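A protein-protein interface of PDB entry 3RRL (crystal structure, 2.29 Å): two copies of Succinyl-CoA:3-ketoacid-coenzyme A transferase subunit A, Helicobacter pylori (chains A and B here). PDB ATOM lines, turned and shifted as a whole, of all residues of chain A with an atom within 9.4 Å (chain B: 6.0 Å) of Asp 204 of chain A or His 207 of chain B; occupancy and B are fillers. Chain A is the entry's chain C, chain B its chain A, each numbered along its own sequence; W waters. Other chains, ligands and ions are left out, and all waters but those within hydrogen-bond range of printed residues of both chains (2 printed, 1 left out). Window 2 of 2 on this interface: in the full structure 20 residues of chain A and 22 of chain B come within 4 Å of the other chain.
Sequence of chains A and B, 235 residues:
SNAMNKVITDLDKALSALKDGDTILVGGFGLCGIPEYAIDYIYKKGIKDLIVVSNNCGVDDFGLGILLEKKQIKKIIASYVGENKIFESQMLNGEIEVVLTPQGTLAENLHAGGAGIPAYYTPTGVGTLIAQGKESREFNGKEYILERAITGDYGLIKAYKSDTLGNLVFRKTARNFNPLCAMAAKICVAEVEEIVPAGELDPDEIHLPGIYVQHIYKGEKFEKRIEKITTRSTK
Among the printed residues, pairs that only touch across the chains: Asp 204 of chain A with Phe 170 of chain B, Asp 204 of chain A with Arg 171 of chain B and Glu 205 of chain A with Glu 205 of chain B.
Asp 204 of chain A touches just these residues of chain B: Phe 170 (3.6 Å), Arg 171 (3.6 Å), Lys 172 (2.9 Å), Arg 175 (3.0 Å) and His 207 (2.8 Å).
Val 169 of chain B touches none of the printed residues of chain A.
Of the printed residues of chain A, Phe 170 of chain B touches Asp 204 (3.6 Å).
Of chain A, only Asp 204 (2.9 Å) comes within 4 Å of Lys 172 of chain B.
Of the printed residues of chain A, Arg 175 of chain B touches Asp 204.
Printed residues of chain A within 4 Å of Glu 205 of chain B: Glu 205 (3.9 Å).
His 207 of chain B touches just one residue of chain A: Asp 204.
The nearest residue of chain A that does not touch His 207 of chain B is Glu 205 of chain A (5.0 Å).
Of the 13 printed residues of chain A, 2 touch a printed residue of chain B.
Printed residues of chain B that touch a printed residue of chain A: Phe 170, Arg 171, Lys 172, Arg 175, Glu 205 and His 207.
Among the printed residues, 6 pairs touch across the chains.
Among the printed residues, Asp or Glu carboxylates within 4 Å of a Lys or Arg side-chain nitrogen of the other chain: Asp 204 of chain A with Arg 175 of chain B (3.0 Å).
Water W1 lies within hydrogen-bond range of OD1 of Asp 204 of chain A (2.6 Å), NE of Arg 175 of chain B (2.6 Å) and O of Lys 172 of chain B (2.8 Å).
Water W2 lies within hydrogen-bond range of the backbone carbonyl oxygen (O) of Glu 205 of chain B (2.7 Å), the backbone carbonyl oxygen (O) of Asp 204 of chain A (2.8 Å) and a ring nitrogen (NE2) of His 207 of chain B (3.3 Å).
NE2 of His 207 of chain B lies within hydrogen-bond range of O of Asp 204 of chain A (2.8 Å).
The backbone NH of Lys 172 of chain B is in hydrogen-bond range of the side-chain carboxylate of Asp 204 of chain A, 2.9 Å away.
The guanidinium group of Arg 175 of chain B is in salt-bridge range of the side-chain carboxylate of Asp 204 of chain A.
Glu 205 of chain A touches its own counterpart, Glu 205 of chain B.
NH1 of Arg 175 of chain B is in hydrogen-bond range of NE2 of His 207 of chain B (3.4 Å).
N of Phe 170 of chain B is in hydrogen-bond range of ND1 of His 207 of chain B, at 2.9 Å.
OD1 of Asp 202 of chain A is in hydrogen-bond range of N of Asp 204 of chain A (2.8 Å).
The backbone carbonyl oxygen of Leu 168 of chain B lies within hydrogen-bond range of the backbone NH of His 207 of chain B (2.9 Å).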
ATOM      1  N   ASN A 167      31.657   1.238  32.995  1.00  0.00           N
ATOM      2  CA  ASN A 167      30.490   0.948  32.171  1.00  0.00           C
ATOM      3  C   ASN A 167      30.816  -0.185  31.199  1.00  0.00           C
ATOM      4  O   ASN A 167      31.821  -0.129  30.491  1.00  0.00           O
ATOM      5  CB  ASN A 167      30.049   2.193  31.400  1.00  0.00           C
ATOM      6  CG  ASN A 167      29.452   3.250  32.299  1.00  0.00           C
ATOM      7  OD1 ASN A 167      28.551   2.963  33.096  1.00  0.00           O
ATOM      8  ND2 ASN A 167      29.955   4.482  32.190  1.00  0.00           N
ATOM      9  N   LEU A 168      29.976  -1.212  31.167  1.00  0.00           N
ATOM     10  CA  LEU A 168      30.256  -2.384  30.323  1.00  0.00           C
ATOM     11  C   LEU A 168      29.227  -2.610  29.219  1.00  0.00           C
ATOM     12  O   LEU A 168      28.030  -2.327  29.382  1.00  0.00           O
ATOM     13  CB  LEU A 168      30.313  -3.661  31.163  1.00  0.00           C
ATOM     14  CG  LEU A 168      31.194  -3.655  32.413  1.00  0.00           C
ATOM     15  CD1 LEU A 168      31.074  -4.985  33.147  1.00  0.00           C
ATOM     16  CD2 LEU A 168      32.642  -3.357  32.049  1.00  0.00           C
ATOM     17  N   VAL A 169      29.705  -3.143  28.101  1.00  0.00           N
ATOM     18  CA  VAL A 169      28.824  -3.755  27.119  1.00  0.00           C
ATOM     19  C   VAL A 169      29.258  -5.199  26.879  1.00  0.00           C
ATOM     20  O   VAL A 169      30.451  -5.513  26.848  1.00  0.00           O
ATOM     21  CB  VAL A 169      28.772  -2.947  25.799  1.00  0.00           C
ATOM     22  CG1 VAL A 169      28.302  -1.531  26.092  1.00  0.00           C
ATOM     23  CG2 VAL A 169      30.126  -2.914  25.136  1.00  0.00           C
ATOM     24  N   ARG A 175      26.811 -12.544  27.186  1.00  0.00           N
ATOM     25  CA  ARG A 175      26.350 -11.831  28.360  1.00  0.00           C
ATOM     26  C   ARG A 175      25.801 -12.710  29.495  1.00  0.00           C
ATOM     27  O   ARG A 175      26.346 -12.706  30.575  1.00  0.00           O
ATOM     28  CB  ARG A 175      25.267 -10.835  27.920  1.00  0.00           C
ATOM     29  CG  ARG A 175      24.694  -9.957  28.994  1.00  0.00           C
ATOM     30  CD  ARG A 175      23.453  -9.179  28.562  1.00  0.00           C
ATOM     31  NE  ARG A 175      23.552  -8.536  27.262  1.00  0.00           N
ATOM     32  CZ  ARG A 175      22.696  -7.642  26.788  1.00  0.00           C
ATOM     33  NH1 ARG A 175      22.853  -7.140  25.598  1.00  0.00           N
ATOM     34  NH2 ARG A 175      21.672  -7.256  27.493  1.00  0.00           N
ATOM     35  N   GLU A 200      33.135   7.569  25.332  1.00  0.00           N
ATOM     36  CA  GLU A 200      33.115   6.853  24.059  1.00  0.00           C
ATOM     37  C   GLU A 200      31.998   5.818  23.976  1.00  0.00           C
ATOM     38  O   GLU A 200      31.630   5.380  22.890  1.00  0.00           O
ATOM     39  CB  GLU A 200      34.478   6.228  23.736  1.00  0.00           C
ATOM     40  CG  GLU A 200      35.512   7.260  23.316  1.00  0.00           C
ATOM     41  CD  GLU A 200      36.713   6.658  22.609  1.00  0.00           C
ATOM     42  OE1 GLU A 200      37.817   7.226  22.747  1.00  0.00           O
ATOM     43  OE2 GLU A 200      36.556   5.633  21.905  1.00  0.00           O
ATOM     44  N   LEU A 201      31.459   5.425  25.122  1.00  0.00           N
ATOM     45  CA  LEU A 201      30.307   4.532  25.136  1.00  0.00           C
ATOM     46  C   LEU A 201      29.040   5.353  25.284  1.00  0.00           C
ATOM     47  O   LEU A 201      28.903   6.114  26.236  1.00  0.00           O
ATOM     48  CB  LEU A 201      30.404   3.539  26.291  1.00  0.00           C
ATOM     49  CG  LEU A 201      31.505   2.488  26.191  1.00  0.00           C
ATOM     50  CD1 LEU A 201      31.310   1.437  27.282  1.00  0.00           C
ATOM     51  CD2 LEU A 201      31.502   1.852  24.797  1.00  0.00           C
ATOM     52  N   ASP A 202      28.111   5.207  24.350  1.00  0.00           N
ATOM     53  CA  ASP A 202      26.859   5.939  24.462  1.00  0.00           C
ATOM     54  C   ASP A 202      26.088   5.517  25.714  1.00  0.00           C
ATOM     55  O   ASP A 202      25.968   4.328  26.006  1.00  0.00           O
ATOM     56  CB  ASP A 202      25.990   5.743  23.225  1.00  0.00           C
ATOM     57  CG  ASP A 202      24.873   6.761  23.146  1.00  0.00           C
ATOM     58  OD1 ASP A 202      23.801   6.542  23.762  1.00  0.00           O
ATOM     59  OD2 ASP A 202      25.085   7.802  22.490  1.00  0.00           O
ATOM     60  N   PRO A 203      25.560   6.503  26.455  1.00  0.00           N
ATOM     61  CA  PRO A 203      24.758   6.295  27.666  1.00  0.00           C
ATOM     62  C   PRO A 203      23.594   5.331  27.430  1.00  0.00           C
ATOM     63  O   PRO A 203      23.215   4.589  28.339  1.00  0.00           O
ATOM     64  CB  PRO A 203      24.209   7.690  27.962  1.00  0.00           C
ATOM     65  CG  PRO A 203      25.164   8.620  27.333  1.00  0.00           C
ATOM     66  CD  PRO A 203      25.671   7.930  26.104  1.00  0.00           C
ATOM     67  N   ASP A 204      23.035   5.340  26.223  1.00  0.00           N
ATOM     68  CA  ASP A 204      21.905   4.472  25.911  1.00  0.00           C
ATOM     69  C   ASP A 204      22.352   3.109  25.339  1.00  0.00           C
ATOM     70  O   ASP A 204      21.521   2.260  25.022  1.00  0.00           O
ATOM     71  CB  ASP A 204      20.933   5.176  24.959  1.00  0.00           C
ATOM     72  CG  ASP A 204      19.870   5.989  25.694  1.00  0.00           C
ATOM     73  OD1 ASP A 204      19.044   5.382  26.425  1.00  0.00           O
ATOM     74  OD2 ASP A 204      19.848   7.234  25.518  1.00  0.00           O
ATOM     75  N   GLU A 205      23.657   2.929  25.160  1.00  0.00           N
ATOM     76  CA  GLU A 205      24.207   1.647  24.713  1.00  0.00           C
ATOM     77  C   GLU A 205      24.840   0.772  25.802  1.00  0.00           C
ATOM     78  O   GLU A 205      25.263  -0.352  25.538  1.00  0.00           O
ATOM     79  CB  GLU A 205      25.187   1.867  23.562  1.00  0.00           C
ATOM     80  CG  GLU A 205      24.561   2.643  22.425  1.00  0.00           C
ATOM     81  CD  GLU A 205      25.451   2.746  21.198  1.00  0.00           C
ATOM     82  OE1 GLU A 205      26.663   2.434  21.289  1.00  0.00           O
ATOM     83  OE2 GLU A 205      24.919   3.145  20.141  1.00  0.00           O
ATOM     84  N   ILE A 206      24.894   1.285  27.022  1.00  0.00           N
ATOM     85  CA  ILE A 206      25.577   0.600  28.108  1.00  0.00           C
ATOM     86  C   ILE A 206      24.697  -0.502  28.702  1.00  0.00           C
ATOM     87  O   ILE A 206      23.521  -0.280  28.989  1.00  0.00           O
ATOM     88  CB  ILE A 206      26.019   1.621  29.182  1.00  0.00           C
ATOM     89  CG1 ILE A 206      27.240   2.403  28.678  1.00  0.00           C
ATOM     90  CG2 ILE A 206      26.310   0.940  30.529  1.00  0.00           C
ATOM     91  CD1 ILE A 206      27.497   3.677  29.441  1.00  0.00           C
ATOM     92  N   HIS A 207      25.249  -1.709  28.825  1.00  0.00           N
ATOM     93  CA  HIS A 207      24.529  -2.811  29.471  1.00  0.00           C
ATOM     94  C   HIS A 207      24.589  -2.787  30.990  1.00  0.00           C
ATOM     95  O   HIS A 207      23.569  -2.935  31.659  1.00  0.00           O
ATOM     96  CB  HIS A 207      25.019  -4.152  28.941  1.00  0.00           C
ATOM     97  CG  HIS A 207      24.766  -4.332  27.480  1.00  0.00           C
ATOM     98  ND1 HIS A 207      25.587  -5.078  26.664  1.00  0.00           N
ATOM     99  CD2 HIS A 207      23.777  -3.849  26.685  1.00  0.00           C
ATOM    100  CE1 HIS A 207      25.114  -5.053  25.428  1.00  0.00           C
ATOM    101  NE2 HIS A 207      24.020  -4.315  25.414  1.00  0.00           N
ATOM    102  N   LEU A 208      25.794  -2.629  31.527  1.00  0.00           N
ATOM    103  CA  LEU A 208      25.998  -2.542  32.970  1.00  0.00           C
ATOM    104  C   LEU A 208      26.654  -1.221  33.374  1.00  0.00           C
ATOM    105  O   LEU A 208      27.793  -0.954  32.979  1.00  0.00           O
ATOM    106  CB  LEU A 208      26.856  -3.712  33.447  1.00  0.00           C
ATOM    107  CG  LEU A 208      26.901  -3.916  34.957  1.00  0.00           C
ATOM    108  CD1 LEU A 208      25.569  -4.469  35.459  1.00  0.00           C
ATOM    109  CD2 LEU A 208      28.043  -4.851  35.312  1.00  0.00           C
ATOM    110  N   LEU B 168      12.316  -2.412  20.694  1.00  0.00           N
ATOM    111  CA  LEU B 168      12.331  -0.989  20.984  1.00  0.00           C
ATOM    112  C   LEU B 168      13.667  -0.508  21.517  1.00  0.00           C
ATOM    113  O   LEU B 168      14.414  -1.257  22.143  1.00  0.00           O
ATOM    114  CB  LEU B 168      11.247  -0.640  22.001  1.00  0.00           C
ATOM    115  CG  LEU B 168       9.828  -1.110  21.709  1.00  0.00           C
ATOM    116  CD1 LEU B 168       8.906  -0.582  22.795  1.00  0.00           C
ATOM    117  CD2 LEU B 168       9.373  -0.655  20.335  1.00  0.00           C
ATOM    118  N   VAL B 169      13.950   0.761  21.257  1.00  0.00           N
ATOM    119  CA  VAL B 169      14.991   1.485  21.965  1.00  0.00           C
ATOM    120  C   VAL B 169      14.360   2.769  22.492  1.00  0.00           C
ATOM    121  O   VAL B 169      13.537   3.390  21.804  1.00  0.00           O
ATOM    122  CB  VAL B 169      16.187   1.821  21.043  1.00  0.00           C
ATOM    123  CG1 VAL B 169      16.878   0.547  20.594  1.00  0.00           C
ATOM    124  CG2 VAL B 169      15.726   2.626  19.827  1.00  0.00           C
ATOM    125  N   PHE B 170      14.721   3.141  23.719  1.00  0.00           N
ATOM    126  CA  PHE B 170      14.303   4.407  24.298  1.00  0.00           C
ATOM    127  C   PHE B 170      15.483   5.364  24.262  1.00  0.00           C
ATOM    128  O   PHE B 170      16.582   4.977  23.889  1.00  0.00           O
ATOM    129  CB  PHE B 170      13.848   4.199  25.747  1.00  0.00           C
ATOM    130  CG  PHE B 170      12.833   3.117  25.896  1.00  0.00           C
ATOM    131  CD1 PHE B 170      13.231   1.787  25.995  1.00  0.00           C
ATOM    132  CD2 PHE B 170      11.482   3.417  25.905  1.00  0.00           C
ATOM    133  CE1 PHE B 170      12.298   0.774  26.106  1.00  0.00           C
ATOM    134  CE2 PHE B 170      10.540   2.409  26.025  1.00  0.00           C
ATOM    135  CZ  PHE B 170      10.949   1.080  26.121  1.00  0.00           C
ATOM    136  N   ARG B 171      15.274   6.609  24.675  1.00  0.00           N
ATOM    137  CA  ARG B 171      16.392   7.547  24.722  1.00  0.00           C
ATOM    138  C   ARG B 171      16.364   8.378  25.999  1.00  0.00           C
ATOM    139  O   ARG B 171      15.299   8.784  26.466  1.00  0.00           O
ATOM    140  CB  ARG B 171      16.447   8.426  23.452  1.00  0.00           C
ATOM    141  CG  ARG B 171      15.340   9.472  23.329  1.00  0.00           C
ATOM    142  CD  ARG B 171      15.376  10.177  21.955  1.00  0.00           C
ATOM    143  NE  ARG B 171      16.549  11.035  21.779  1.00  0.00           N
ATOM    144  CZ  ARG B 171      16.649  12.269  22.272  1.00  0.00           C
ATOM    145  NH1 ARG B 171      15.651  12.793  22.970  1.00  0.00           N
ATOM    146  NH2 ARG B 171      17.748  12.983  22.073  1.00  0.00           N
ATOM    147  N   LYS B 172      17.523   8.543  26.610  1.00  0.00           N
ATOM    148  CA  LYS B 172      17.664   9.289  27.851  1.00  0.00           C
ATOM    149  C   LYS B 172      16.784   8.799  29.003  1.00  0.00           C
ATOM    150  O   LYS B 172      16.636   7.624  29.228  1.00  0.00           O
ATOM    151  CB  LYS B 172      17.443  10.782  27.621  1.00  0.00           C
ATOM    152  CG  LYS B 172      17.772  11.277  26.245  1.00  0.00           C
ATOM    153  CD  LYS B 172      19.169  10.904  25.838  1.00  0.00           C
ATOM    154  CE  LYS B 172      19.847  12.017  25.093  1.00  0.00           C
ATOM    155  NZ  LYS B 172      21.032  11.559  24.352  1.00  0.00           N
ATOM    156  N   ARG B 175      12.963   6.722  29.074  1.00  0.00           N
ATOM    157  CA  ARG B 175      12.700   5.305  29.261  1.00  0.00           C
ATOM    158  C   ARG B 175      11.917   4.949  30.520  1.00  0.00           C
ATOM    159  O   ARG B 175      10.853   4.383  30.424  1.00  0.00           O
ATOM    160  CB  ARG B 175      14.052   4.587  29.301  1.00  0.00           C
ATOM    161  CG  ARG B 175      13.995   3.094  29.232  1.00  0.00           C
ATOM    162  CD  ARG B 175      15.308   2.421  29.594  1.00  0.00           C
ATOM    163  NE  ARG B 175      16.465   3.004  28.936  1.00  0.00           N
ATOM    164  CZ  ARG B 175      17.607   2.364  28.727  1.00  0.00           C
ATOM    165  NH1 ARG B 175      18.610   2.968  28.139  1.00  0.00           N
ATOM    166  NH2 ARG B 175      17.742   1.116  29.105  1.00  0.00           N
ATOM    167  N   PRO B 179       9.342   0.228  29.681  1.00  0.00           N
ATOM    168  CA  PRO B 179       9.515  -1.211  29.431  1.00  0.00           C
ATOM    169  C   PRO B 179       8.780  -2.078  30.467  1.00  0.00           C
ATOM    170  O   PRO B 179       8.291  -3.161  30.131  1.00  0.00           O
ATOM    171  CB  PRO B 179      11.034  -1.404  29.516  1.00  0.00           C
ATOM    172  CG  PRO B 179      11.501  -0.296  30.408  1.00  0.00           C
ATOM    173  CD  PRO B 179      10.597   0.876  30.105  1.00  0.00           C
ATOM    174  N   GLU B 205      21.942  -3.582  20.981  1.00  0.00           N
ATOM    175  CA  GLU B 205      21.507  -2.242  21.372  1.00  0.00           C
ATOM    176  C   GLU B 205      20.025  -2.148  21.736  1.00  0.00           C
ATOM    177  O   GLU B 205      19.560  -1.113  22.201  1.00  0.00           O
ATOM    178  CB  GLU B 205      21.866  -1.229  20.278  1.00  0.00           C
ATOM    179  CG  GLU B 205      23.360  -1.208  19.961  1.00  0.00           C
ATOM    180  CD  GLU B 205      23.713  -0.338  18.758  1.00  0.00           C
ATOM    181  OE1 GLU B 205      22.846   0.444  18.297  1.00  0.00           O
ATOM    182  OE2 GLU B 205      24.865  -0.439  18.276  1.00  0.00           O
ATOM    183  N   ILE B 206      19.296  -3.236  21.539  1.00  0.00           N
ATOM    184  CA  ILE B 206      17.855  -3.249  21.761  1.00  0.00           C
ATOM    185  C   ILE B 206      17.523  -3.217  23.254  1.00  0.00           C
ATOM    186  O   ILE B 206      18.092  -3.972  24.038  1.00  0.00           O
ATOM    187  CB  ILE B 206      17.235  -4.485  21.090  1.00  0.00           C
ATOM    188  CG1 ILE B 206      17.152  -4.252  19.581  1.00  0.00           C
ATOM    189  CG2 ILE B 206      15.865  -4.793  21.669  1.00  0.00           C
ATOM    190  CD1 ILE B 206      17.036  -5.522  18.767  1.00  0.00           C
ATOM    191  N   HIS B 207      16.664  -2.289  23.659  1.00  0.00           N
ATOM    192  CA  HIS B 207      16.252  -2.207  25.061  1.00  0.00           C
ATOM    193  C   HIS B 207      15.121  -3.170  25.413  1.00  0.00           C
ATOM    194  O   HIS B 207      15.187  -3.860  26.415  1.00  0.00           O
ATOM    195  CB  HIS B 207      15.871  -0.774  25.440  1.00  0.00           C
ATOM    196  CG  HIS B 207      16.994   0.207  25.294  1.00  0.00           C
ATOM    197  ND1 HIS B 207      16.799   1.509  24.870  1.00  0.00           N
ATOM    198  CD2 HIS B 207      18.326   0.075  25.512  1.00  0.00           C
ATOM    199  CE1 HIS B 207      17.964   2.133  24.828  1.00  0.00           C
ATOM    200  NE2 HIS B 207      18.905   1.287  25.215  1.00  0.00           N
ATOM    201  N   LEU B 208      14.066  -3.187  24.604  1.00  0.00           N
ATOM    202  CA  LEU B 208      12.919  -4.053  24.876  1.00  0.00           C
ATOM    203  C   LEU B 208      12.616  -5.030  23.752  1.00  0.00           C
ATOM    204  O   LEU B 208      12.153  -4.612  22.693  1.00  0.00           O
ATOM    205  CB  LEU B 208      11.672  -3.221  25.162  1.00  0.00           C
ATOM    206  CG  LEU B 208      10.462  -4.040  25.602  1.00  0.00           C
ATOM    207  CD1 LEU B 208      10.608  -4.465  27.071  1.00  0.00           C
ATOM    208  CD2 LEU B 208       9.170  -3.257  25.365  1.00  0.00           C
ATOM    209  N   PRO B 209      12.853  -6.333  23.979  1.00  0.00           N
ATOM    210  CA  PRO B 209      12.580  -7.319  22.927  1.00  0.00           C
ATOM    211  C   PRO B 209      11.134  -7.259  22.456  1.00  0.00           C
ATOM    212  O   PRO B 209      10.231  -7.020  23.257  1.00  0.00           O
ATOM    213  CB  PRO B 209      12.886  -8.654  23.609  1.00  0.00           C
ATOM    214  CG  PRO B 209      13.936  -8.306  24.642  1.00  0.00           C
ATOM    215  CD  PRO B 209      13.527  -6.934  25.146  1.00  0.00           C
HETATM  216  O   HOH W   1      16.783   5.298  27.651  1.00  0.00           O
HETATM  217  O   HOH W   2      20.821   1.219  22.471  1.00  0.00           O
